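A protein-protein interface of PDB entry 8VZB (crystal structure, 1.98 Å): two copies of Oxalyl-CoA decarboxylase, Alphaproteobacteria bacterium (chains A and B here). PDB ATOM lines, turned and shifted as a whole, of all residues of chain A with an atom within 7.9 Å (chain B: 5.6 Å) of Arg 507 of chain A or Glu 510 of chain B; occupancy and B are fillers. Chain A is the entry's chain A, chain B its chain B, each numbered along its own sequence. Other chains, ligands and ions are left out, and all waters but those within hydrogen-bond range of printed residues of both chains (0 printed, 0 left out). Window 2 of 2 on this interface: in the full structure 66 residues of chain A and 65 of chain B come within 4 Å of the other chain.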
ATOM      1  N   PHE A 461      20.521  -1.169  36.435  1.00  0.00           N
ATOM      2  CA  PHE A 461      20.613  -2.596  36.720  1.00  0.00           C
ATOM      3  C   PHE A 461      21.929  -3.168  36.219  1.00  0.00           C
ATOM      4  O   PHE A 461      22.473  -4.095  36.829  1.00  0.00           O
ATOM      5  CB  PHE A 461      19.434  -3.342  36.093  1.00  0.00           C
ATOM      6  CG  PHE A 461      19.291  -4.763  36.568  1.00  0.00           C
ATOM      7  CD1 PHE A 461      19.980  -5.793  35.944  1.00  0.00           C
ATOM      8  CD2 PHE A 461      18.468  -5.065  37.639  1.00  0.00           C
ATOM      9  CE1 PHE A 461      19.856  -7.099  36.387  1.00  0.00           C
ATOM     10  CE2 PHE A 461      18.333  -6.374  38.088  1.00  0.00           C
ATOM     11  CZ  PHE A 461      19.026  -7.390  37.459  1.00  0.00           C
ATOM     12  N   ASP A 502       1.941  -4.487  28.657  1.00  0.00           N
ATOM     13  CA  ASP A 502       2.471  -5.792  28.289  1.00  0.00           C
ATOM     14  C   ASP A 502       3.994  -5.827  28.234  1.00  0.00           C
ATOM     15  O   ASP A 502       4.560  -6.839  27.807  1.00  0.00           O
ATOM     16  CB  ASP A 502       1.894  -6.234  26.943  1.00  0.00           C
ATOM     17  CG  ASP A 502       0.412  -6.536  27.020  1.00  0.00           C
ATOM     18  OD1 ASP A 502      -0.037  -7.010  28.086  1.00  0.00           O
ATOM     19  OD2 ASP A 502      -0.303  -6.302  26.021  1.00  0.00           O
ATOM     20  N   ALA A 503       4.664  -4.760  28.663  1.00  0.00           N
ATOM     21  CA  ALA A 503       6.120  -4.730  28.617  1.00  0.00           C
ATOM     22  C   ALA A 503       6.708  -5.845  29.474  1.00  0.00           C
ATOM     23  O   ALA A 503       6.193  -6.169  30.549  1.00  0.00           O
ATOM     24  CB  ALA A 503       6.642  -3.370  29.084  1.00  0.00           C
ATOM     25  N   ARG A 504       7.785  -6.446  28.979  1.00  0.00           N
ATOM     26  CA  ARG A 504       8.489  -7.514  29.675  1.00  0.00           C
ATOM     27  C   ARG A 504       9.786  -6.951  30.254  1.00  0.00           C
ATOM     28  O   ARG A 504      10.894  -7.295  29.834  1.00  0.00           O
ATOM     29  CB  ARG A 504       8.744  -8.692  28.717  1.00  0.00           C
ATOM     30  CG  ARG A 504       7.479  -9.287  28.092  1.00  0.00           C
ATOM     31  CD  ARG A 504       6.655 -10.047  29.124  1.00  0.00           C
ATOM     32  NE  ARG A 504       7.387 -11.189  29.660  1.00  0.00           N
ATOM     33  CZ  ARG A 504       7.204 -12.446  29.279  1.00  0.00           C
ATOM     34  NH1 ARG A 504       6.288 -12.771  28.380  1.00  0.00           N
ATOM     35  NH2 ARG A 504       7.954 -13.403  29.818  1.00  0.00           N
ATOM     36  N   TYR A 505       9.626  -6.062  31.240  1.00  0.00           N
ATOM     37  CA  TYR A 505      10.772  -5.396  31.853  1.00  0.00           C
ATOM     38  C   TYR A 505      11.797  -6.386  32.393  1.00  0.00           C
ATOM     39  O   TYR A 505      12.996  -6.083  32.411  1.00  0.00           O
ATOM     40  CB  TYR A 505      10.308  -4.482  32.987  1.00  0.00           C
ATOM     41  CG  TYR A 505       9.538  -3.259  32.545  1.00  0.00           C
ATOM     42  CD1 TYR A 505      10.183  -2.198  31.923  1.00  0.00           C
ATOM     43  CD2 TYR A 505       8.171  -3.153  32.772  1.00  0.00           C
ATOM     44  CE1 TYR A 505       9.488  -1.070  31.525  1.00  0.00           C
ATOM     45  CE2 TYR A 505       7.466  -2.028  32.380  1.00  0.00           C
ATOM     46  CZ  TYR A 505       8.131  -0.989  31.755  1.00  0.00           C
ATOM     47  OH  TYR A 505       7.437   0.132  31.357  1.00  0.00           O
ATOM     48  N   GLU A 506      11.352  -7.564  32.837  1.00  0.00           N
ATOM     49  CA  GLU A 506      12.259  -8.512  33.475  1.00  0.00           C
ATOM     50  C   GLU A 506      13.361  -8.984  32.534  1.00  0.00           C
ATOM     51  O   GLU A 506      14.424  -9.402  33.005  1.00  0.00           O
ATOM     52  CB  GLU A 506      11.479  -9.714  34.018  1.00  0.00           C
ATOM     53  CG  GLU A 506      11.119 -10.768  32.978  1.00  0.00           C
ATOM     54  CD  GLU A 506       9.907 -10.399  32.137  1.00  0.00           C
ATOM     55  OE1 GLU A 506       9.223  -9.401  32.461  1.00  0.00           O
ATOM     56  OE2 GLU A 506       9.636 -11.112  31.150  1.00  0.00           O
ATOM     57  N   ARG A 507      13.141  -8.918  31.220  1.00  0.00           N
ATOM     58  CA  ARG A 507      14.183  -9.291  30.274  1.00  0.00           C
ATOM     59  C   ARG A 507      15.368  -8.338  30.304  1.00  0.00           C
ATOM     60  O   ARG A 507      16.426  -8.675  29.760  1.00  0.00           O
ATOM     61  CB  ARG A 507      13.602  -9.372  28.863  1.00  0.00           C
ATOM     62  CG  ARG A 507      12.700 -10.585  28.668  1.00  0.00           C
ATOM     63  CD  ARG A 507      11.887 -10.497  27.393  1.00  0.00           C
ATOM     64  NE  ARG A 507      10.934 -11.597  27.298  1.00  0.00           N
ATOM     65  CZ  ARG A 507      10.003 -11.702  26.360  1.00  0.00           C
ATOM     66  NH1 ARG A 507       9.863 -10.783  25.419  1.00  0.00           N
ATOM     67  NH2 ARG A 507       9.193 -12.757  26.367  1.00  0.00           N
ATOM     68  N   ILE A 508      15.220  -7.163  30.918  1.00  0.00           N
ATOM     69  CA  ILE A 508      16.365  -6.282  31.105  1.00  0.00           C
ATOM     70  C   ILE A 508      17.382  -6.925  32.039  1.00  0.00           C
ATOM     71  O   ILE A 508      18.597  -6.783  31.852  1.00  0.00           O
ATOM     72  CB  ILE A 508      15.898  -4.910  31.622  1.00  0.00           C
ATOM     73  CG1 ILE A 508      15.168  -4.150  30.510  1.00  0.00           C
ATOM     74  CG2 ILE A 508      17.075  -4.109  32.155  1.00  0.00           C
ATOM     75  CD1 ILE A 508      14.266  -3.046  31.019  1.00  0.00           C
ATOM     76  N   ALA A 509      16.906  -7.654  33.050  1.00  0.00           N
ATOM     77  CA  ALA A 509      17.819  -8.378  33.926  1.00  0.00           C
ATOM     78  C   ALA A 509      18.636  -9.394  33.141  1.00  0.00           C
ATOM     79  O   ALA A 509      19.847  -9.530  33.358  1.00  0.00           O
ATOM     80  CB  ALA A 509      17.041  -9.068  35.044  1.00  0.00           C
ATOM     81  N   GLU A 510      17.993 -10.103  32.213  1.00  0.00           N
ATOM     82  CA  GLU A 510      18.682 -11.100  31.406  1.00  0.00           C
ATOM     83  C   GLU A 510      19.665 -10.473  30.427  1.00  0.00           C
ATOM     84  O   GLU A 510      20.574 -11.162  29.948  1.00  0.00           O
ATOM     85  CB  GLU A 510      17.649 -11.959  30.672  1.00  0.00           C
ATOM     86  CG  GLU A 510      16.747 -12.742  31.636  1.00  0.00           C
ATOM     87  CD  GLU A 510      15.498 -13.306  30.980  1.00  0.00           C
ATOM     88  OE1 GLU A 510      15.199 -12.935  29.826  1.00  0.00           O
ATOM     89  OE2 GLU A 510      14.807 -14.124  31.628  1.00  0.00           O
ATOM     90  N   ALA A 511      19.512  -9.182  30.124  1.00  0.00           N
ATOM     91  CA  ALA A 511      20.515  -8.492  29.322  1.00  0.00           C
ATOM     92  C   ALA A 511      21.852  -8.401  30.046  1.00  0.00           C
ATOM     93  O   ALA A 511      22.900  -8.330  29.394  1.00  0.00           O
ATOM     94  CB  ALA A 511      20.025  -7.092  28.952  1.00  0.00           C
ATOM     95  N   PHE A 512      21.844  -8.413  31.385  1.00  0.00           N
ATOM     96  CA  PHE A 512      23.055  -8.149  32.156  1.00  0.00           C
ATOM     97  C   PHE A 512      23.380  -9.262  33.149  1.00  0.00           C
ATOM     98  O   PHE A 512      24.082  -9.013  34.134  1.00  0.00           O
ATOM     99  CB  PHE A 512      22.939  -6.805  32.882  1.00  0.00           C
ATOM    100  CG  PHE A 512      22.578  -5.668  31.973  1.00  0.00           C
ATOM    101  CD1 PHE A 512      23.432  -5.288  30.954  1.00  0.00           C
ATOM    102  CD2 PHE A 512      21.380  -4.988  32.128  1.00  0.00           C
ATOM    103  CE1 PHE A 512      23.105  -4.248  30.107  1.00  0.00           C
ATOM    104  CE2 PHE A 512      21.047  -3.942  31.284  1.00  0.00           C
ATOM    105  CZ  PHE A 512      21.912  -3.572  30.271  1.00  0.00           C
ATOM    106  N   GLY A 513      22.904 -10.484  32.909  1.00  0.00           N
ATOM    107  CA  GLY A 513      23.276 -11.623  33.725  1.00  0.00           C
ATOM    108  C   GLY A 513      22.464 -11.823  34.985  1.00  0.00           C
ATOM    109  O   GLY A 513      22.831 -12.667  35.811  1.00  0.00           O
ATOM    110  N   GLY A 514      21.382 -11.070  35.172  1.00  0.00           N
ATOM    111  CA  GLY A 514      20.520 -11.254  36.315  1.00  0.00           C
ATOM    112  C   GLY A 514      19.354 -12.174  36.000  1.00  0.00           C
ATOM    113  O   GLY A 514      19.142 -12.601  34.865  1.00  0.00           O
ATOM    114  N   ALA A 515      18.584 -12.481  37.039  1.00  0.00           N
ATOM    115  CA  ALA A 515      17.410 -13.334  36.900  1.00  0.00           C
ATOM    116  C   ALA A 515      16.175 -12.474  36.661  1.00  0.00           C
ATOM    117  O   ALA A 515      15.972 -11.466  37.345  1.00  0.00           O
ATOM    118  CB  ALA A 515      17.221 -14.204  38.144  1.00  0.00           C
ATOM    119  N   GLY A 516      15.362 -12.871  35.691  1.00  0.00           N
ATOM    120  CA  GLY A 516      14.129 -12.166  35.371  1.00  0.00           C
ATOM    121  C   GLY A 516      12.920 -13.055  35.598  1.00  0.00           C
ATOM    122  O   GLY A 516      12.946 -14.242  35.267  1.00  0.00           O
ATOM    123  N   PHE A 517      11.863 -12.471  36.163  1.00  0.00           N
ATOM    124  CA  PHE A 517      10.637 -13.192  36.473  1.00  0.00           C
ATOM    125  C   PHE A 517       9.436 -12.359  36.057  1.00  0.00           C
ATOM    126  O   PHE A 517       9.389 -11.152  36.310  1.00  0.00           O
ATOM    127  CB  PHE A 517      10.542 -13.526  37.967  1.00  0.00           C
ATOM    128  CG  PHE A 517      11.712 -14.312  38.485  1.00  0.00           C
ATOM    129  CD1 PHE A 517      12.852 -13.667  38.937  1.00  0.00           C
ATOM    130  CD2 PHE A 517      11.675 -15.695  38.512  1.00  0.00           C
ATOM    131  CE1 PHE A 517      13.931 -14.385  39.407  1.00  0.00           C
ATOM    132  CE2 PHE A 517      12.751 -16.419  38.982  1.00  0.00           C
ATOM    133  CZ  PHE A 517      13.881 -15.763  39.431  1.00  0.00           C
ATOM    134  N   TYR A 518       8.468 -13.010  35.419  1.00  0.00           N
ATOM    135  CA  TYR A 518       7.249 -12.361  34.954  1.00  0.00           C
ATOM    136  C   TYR A 518       6.061 -13.003  35.652  1.00  0.00           C
ATOM    137  O   TYR A 518       5.915 -14.229  35.629  1.00  0.00           O
ATOM    138  CB  TYR A 518       7.108 -12.481  33.435  1.00  0.00           C
ATOM    139  CG  TYR A 518       5.983 -11.660  32.841  1.00  0.00           C
ATOM    140  CD1 TYR A 518       5.786 -10.337  33.220  1.00  0.00           C
ATOM    141  CD2 TYR A 518       5.132 -12.201  31.882  1.00  0.00           C
ATOM    142  CE1 TYR A 518       4.767  -9.579  32.672  1.00  0.00           C
ATOM    143  CE2 TYR A 518       4.109 -11.450  31.324  1.00  0.00           C
ATOM    144  CZ  TYR A 518       3.933 -10.138  31.723  1.00  0.00           C
ATOM    145  OH  TYR A 518       2.920  -9.382  31.175  1.00  0.00           O
ATOM    146  N   ILE A 540      14.957  -9.018  38.655  1.00  0.00           N
ATOM    147  CA  ILE A 540      13.775  -8.209  38.388  1.00  0.00           C
ATOM    148  C   ILE A 540      12.558  -9.119  38.397  1.00  0.00           C
ATOM    149  O   ILE A 540      12.524 -10.124  37.678  1.00  0.00           O
ATOM    150  CB  ILE A 540      13.866  -7.463  37.043  1.00  0.00           C
ATOM    151  CG1 ILE A 540      14.935  -6.374  37.092  1.00  0.00           C
ATOM    152  CG2 ILE A 540      12.513  -6.855  36.684  1.00  0.00           C
ATOM    153  CD1 ILE A 540      15.086  -5.634  35.783  1.00  0.00           C
ATOM    154  N   ASN A 542       8.759  -8.707  37.405  1.00  0.00           N
ATOM    155  CA  ASN A 542       7.822  -7.848  36.690  1.00  0.00           C
ATOM    156  C   ASN A 542       6.418  -8.394  36.926  1.00  0.00           C
ATOM    157  O   ASN A 542       6.074  -9.470  36.431  1.00  0.00           O
ATOM    158  CB  ASN A 542       8.171  -7.802  35.203  1.00  0.00           C
ATOM    159  CG  ASN A 542       7.274  -6.867  34.409  1.00  0.00           C
ATOM    160  OD1 ASN A 542       6.651  -5.960  34.960  1.00  0.00           O
ATOM    161  ND2 ASN A 542       7.210  -7.085  33.098  1.00  0.00           N
ATOM    162  N   PHE B 461      13.942   3.305  24.349  1.00  0.00           N
ATOM    163  CA  PHE B 461      13.523   2.351  23.329  1.00  0.00           C
ATOM    164  C   PHE B 461      12.066   1.945  23.521  1.00  0.00           C
ATOM    165  O   PHE B 461      11.367   1.669  22.539  1.00  0.00           O
ATOM    166  CB  PHE B 461      14.434   1.118  23.341  1.00  0.00           C
ATOM    167  CG  PHE B 461      14.184   0.162  22.197  1.00  0.00           C
ATOM    168  CD1 PHE B 461      13.202  -0.814  22.287  1.00  0.00           C
ATOM    169  CD2 PHE B 461      14.934   0.240  21.035  1.00  0.00           C
ATOM    170  CE1 PHE B 461      12.968  -1.687  21.237  1.00  0.00           C
ATOM    171  CE2 PHE B 461      14.712  -0.633  19.982  1.00  0.00           C
ATOM    172  CZ  PHE B 461      13.727  -1.600  20.085  1.00  0.00           C
ATOM    173  N   GLU B 506      20.783  -6.127  23.275  1.00  0.00           N
ATOM    174  CA  GLU B 506      19.699  -6.348  22.325  1.00  0.00           C
ATOM    175  C   GLU B 506      18.467  -6.943  22.991  1.00  0.00           C
ATOM    176  O   GLU B 506      17.358  -6.798  22.463  1.00  0.00           O
ATOM    177  CB  GLU B 506      20.171  -7.251  21.181  1.00  0.00           C
ATOM    178  CG  GLU B 506      20.258  -8.737  21.524  1.00  0.00           C
ATOM    179  CD  GLU B 506      21.461  -9.090  22.383  1.00  0.00           C
ATOM    180  OE1 GLU B 506      22.319  -8.211  22.628  1.00  0.00           O
ATOM    181  OE2 GLU B 506      21.551 -10.262  22.811  1.00  0.00           O
ATOM    182  N   ARG B 507      18.629  -7.596  24.145  1.00  0.00           N
ATOM    183  CA  ARG B 507      17.475  -8.138  24.845  1.00  0.00           C
ATOM    184  C   ARG B 507      16.578  -7.042  25.402  1.00  0.00           C
ATOM    185  O   ARG B 507      15.409  -7.309  25.707  1.00  0.00           O
ATOM    186  CB  ARG B 507      17.938  -9.080  25.955  1.00  0.00           C
ATOM    187  CG  ARG B 507      18.523 -10.374  25.415  1.00  0.00           C
ATOM    188  CD  ARG B 507      19.150 -11.224  26.503  1.00  0.00           C
ATOM    189  NE  ARG B 507      19.716 -12.450  25.958  1.00  0.00           N
ATOM    190  CZ  ARG B 507      20.549 -13.246  26.613  1.00  0.00           C
ATOM    191  NH1 ARG B 507      20.945 -12.967  27.844  1.00  0.00           N
ATOM    192  NH2 ARG B 507      21.004 -14.344  26.015  1.00  0.00           N
ATOM    193  N   ILE B 508      17.092  -5.818  25.536  1.00  0.00           N
ATOM    194  CA  ILE B 508      16.236  -4.693  25.893  1.00  0.00           C
ATOM    195  C   ILE B 508      15.184  -4.458  24.817  1.00  0.00           C
ATOM    196  O   ILE B 508      14.045  -4.078  25.119  1.00  0.00           O
ATOM    197  CB  ILE B 508      17.094  -3.437  26.140  1.00  0.00           C
ATOM    198  CG1 ILE B 508      17.984  -3.646  27.368  1.00  0.00           C
ATOM    199  CG2 ILE B 508      16.216  -2.200  26.300  1.00  0.00           C
ATOM    200  CD1 ILE B 508      19.054  -2.597  27.538  1.00  0.00           C
ATOM    201  N   ALA B 509      15.536  -4.697  23.550  1.00  0.00           N
ATOM    202  CA  ALA B 509      14.559  -4.554  22.477  1.00  0.00           C
ATOM    203  C   ALA B 509      13.440  -5.576  22.613  1.00  0.00           C
ATOM    204  O   ALA B 509      12.281  -5.286  22.297  1.00  0.00           O
ATOM    205  CB  ALA B 509      15.241  -4.689  21.115  1.00  0.00           C
ATOM    206  N   GLU B 510      13.769  -6.781  23.083  1.00  0.00           N
ATOM    207  CA  GLU B 510      12.767  -7.825  23.252  1.00  0.00           C
ATOM    208  C   GLU B 510      11.895  -7.605  24.478  1.00  0.00           C
ATOM    209  O   GLU B 510      10.829  -8.220  24.583  1.00  0.00           O
ATOM    210  CB  GLU B 510      13.450  -9.193  23.328  1.00  0.00           C
ATOM    211  CG  GLU B 510      14.062  -9.612  22.004  1.00  0.00           C
ATOM    212  CD  GLU B 510      15.101 -10.704  22.151  1.00  0.00           C
ATOM    213  OE1 GLU B 510      15.459 -11.040  23.301  1.00  0.00           O
ATOM    214  OE2 GLU B 510      15.563 -11.221  21.110  1.00  0.00           O
ATOM    215  N   ALA B 511      12.321  -6.746  25.406  1.00  0.00           N
ATOM    216  CA  ALA B 511      11.456  -6.391  26.523  1.00  0.00           C
ATOM    217  C   ALA B 511      10.232  -5.612  26.060  1.00  0.00           C
ATOM    218  O   ALA B 511       9.175  -5.679  26.699  1.00  0.00           O
ATOM    219  CB  ALA B 511      12.240  -5.577  27.554  1.00  0.00           C
ATOM    220  N   PHE B 512      10.348  -4.878  24.953  1.00  0.00           N
ATOM    221  CA  PHE B 512       9.300  -3.963  24.518  1.00  0.00           C
ATOM    222  C   PHE B 512       8.766  -4.306  23.132  1.00  0.00           C
ATOM    223  O   PHE B 512       8.148  -3.460  22.478  1.00  0.00           O
ATOM    224  CB  PHE B 512       9.817  -2.522  24.569  1.00  0.00           C
ATOM    225  CG  PHE B 512      10.447  -2.159  25.887  1.00  0.00           C
ATOM    226  CD1 PHE B 512       9.696  -2.167  27.055  1.00  0.00           C
ATOM    227  CD2 PHE B 512      11.788  -1.821  25.963  1.00  0.00           C
ATOM    228  CE1 PHE B 512      10.269  -1.840  28.272  1.00  0.00           C
ATOM    229  CE2 PHE B 512      12.369  -1.491  27.179  1.00  0.00           C
ATOM    230  CZ  PHE B 512      11.609  -1.501  28.335  1.00  0.00           C
ATOM    231  N   GLY B 513       8.987  -5.534  22.672  1.00  0.00           N
ATOM    232  CA  GLY B 513       8.418  -5.972  21.415  1.00  0.00           C
ATOM    233  C   GLY B 513       9.224  -5.626  20.186  1.00  0.00           C
ATOM    234  O   GLY B 513       8.727  -5.805  19.070  1.00  0.00           O
ATOM    235  N   GLY B 514      10.447  -5.123  20.351  1.00  0.00           N
ATOM    236  CA  GLY B 514      11.322  -4.866  19.229  1.00  0.00           C
ATOM    237  C   GLY B 514      12.123  -6.100  18.856  1.00  0.00           C
ATOM    238  O   GLY B 514      12.028  -7.154  19.483  1.00  0.00           O
ATOM    239  N   ALA B 515      12.924  -5.960  17.806  1.00  0.00           N
ATOM    240  CA  ALA B 515      13.756  -7.050  17.321  1.00  0.00           C
ATOM    241  C   ALA B 515      15.171  -6.885  17.859  1.00  0.00           C
ATOM    242  O   ALA B 515      15.746  -5.794  17.775  1.00  0.00           O
ATOM    243  CB  ALA B 515      13.767  -7.093  15.793  1.00  0.00           C
ATOM    244  N   GLY B 516      15.725  -7.960  18.413  1.00  0.00           N
ATOM    245  CA  GLY B 516      17.078  -7.928  18.933  1.00  0.00           C
ATOM    246  C   GLY B 516      18.049  -8.815  18.180  1.00  0.00           C
ATOM    247  O   GLY B 516      17.744  -9.971  17.877  1.00  0.00           O
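Of the printed residues of chain B, Ala 503 of chain A touches Ala 511 (3.7 Å) and Phe 512 (3.9 Å). Printed residues of chain B within 4 Å of Arg 504 of chain A: Ala 511 (2.8 Å). Of the printed residues of chain B, Tyr 505 of chain A touches Phe 512 (3.4 Å). Arg 507 of chain A touches just one residue of chain B: Glu 510. Printed residues of chain B within 4 Å of Glu 510 of chain A: Arg 507 (2.8 Å). Glu 510 of chain B touches just one residue of chain A: Arg 507 (2.9 Å). Of chain A, only Ala 503 (3.7 Å) and Arg 504 (2.8 Å) come within 4 Å of Ala 511 of chain B. Of the printed residues of chain A, Phe 512 of chain B touches Ala 503 and Tyr 505.
The side-chain carboxylate (OE2) of Glu 506 of chain A is in salt-bridge range of the guanidinium group (NE) of Arg 504 of chain A, at 2.7 Å. ND2 of Asn 542 of chain A sits close to N of Tyr 505 of chain A, at 3.2 Å. The side-chain amide nitrogen of Asn 542 of chain A is in hydrogen-bond range of the backbone carbonyl oxygen of Ala 503 of chain A (2.9 Å).
Ala 503 of chain A touches Ala 511 of chain B. CB of Ala 503 of chain A touches CD1 of Phe 512 of chain B, 3.9 Å away. Phe 512 of chain B touches Tyr 505 of chain A (CE1 to CE1, 3.4 Å).
Hydrophobic or aromatic side chains of chain A that line the printed part of chain B: Ala 503 and Tyr 505. Hydrophobic or aromatic side chains of chain B that line the printed part of chain A: Ala 511 and Phe 512.
The backbone carbonyl oxygen of Glu 510 of chain B sits at hydrogen-bond distance from the guanidinium group of Arg 507 of chain A, at 2.9 Å. The backbone NH of Arg 504 of chain A sits at hydrogen-bond distance from the backbone carbonyl oxygen of Ala 511 of chain B, 2.8 Å away. O of Glu 510 of chain A lies within hydrogen-bond range of NH1 of Arg 507 of chain B (2.8 Å).
Arg 507 of chain A touches Glu 510 of chain B, and with the chains exchanged Glu 510 of chain A touches Arg 507 of chain B.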
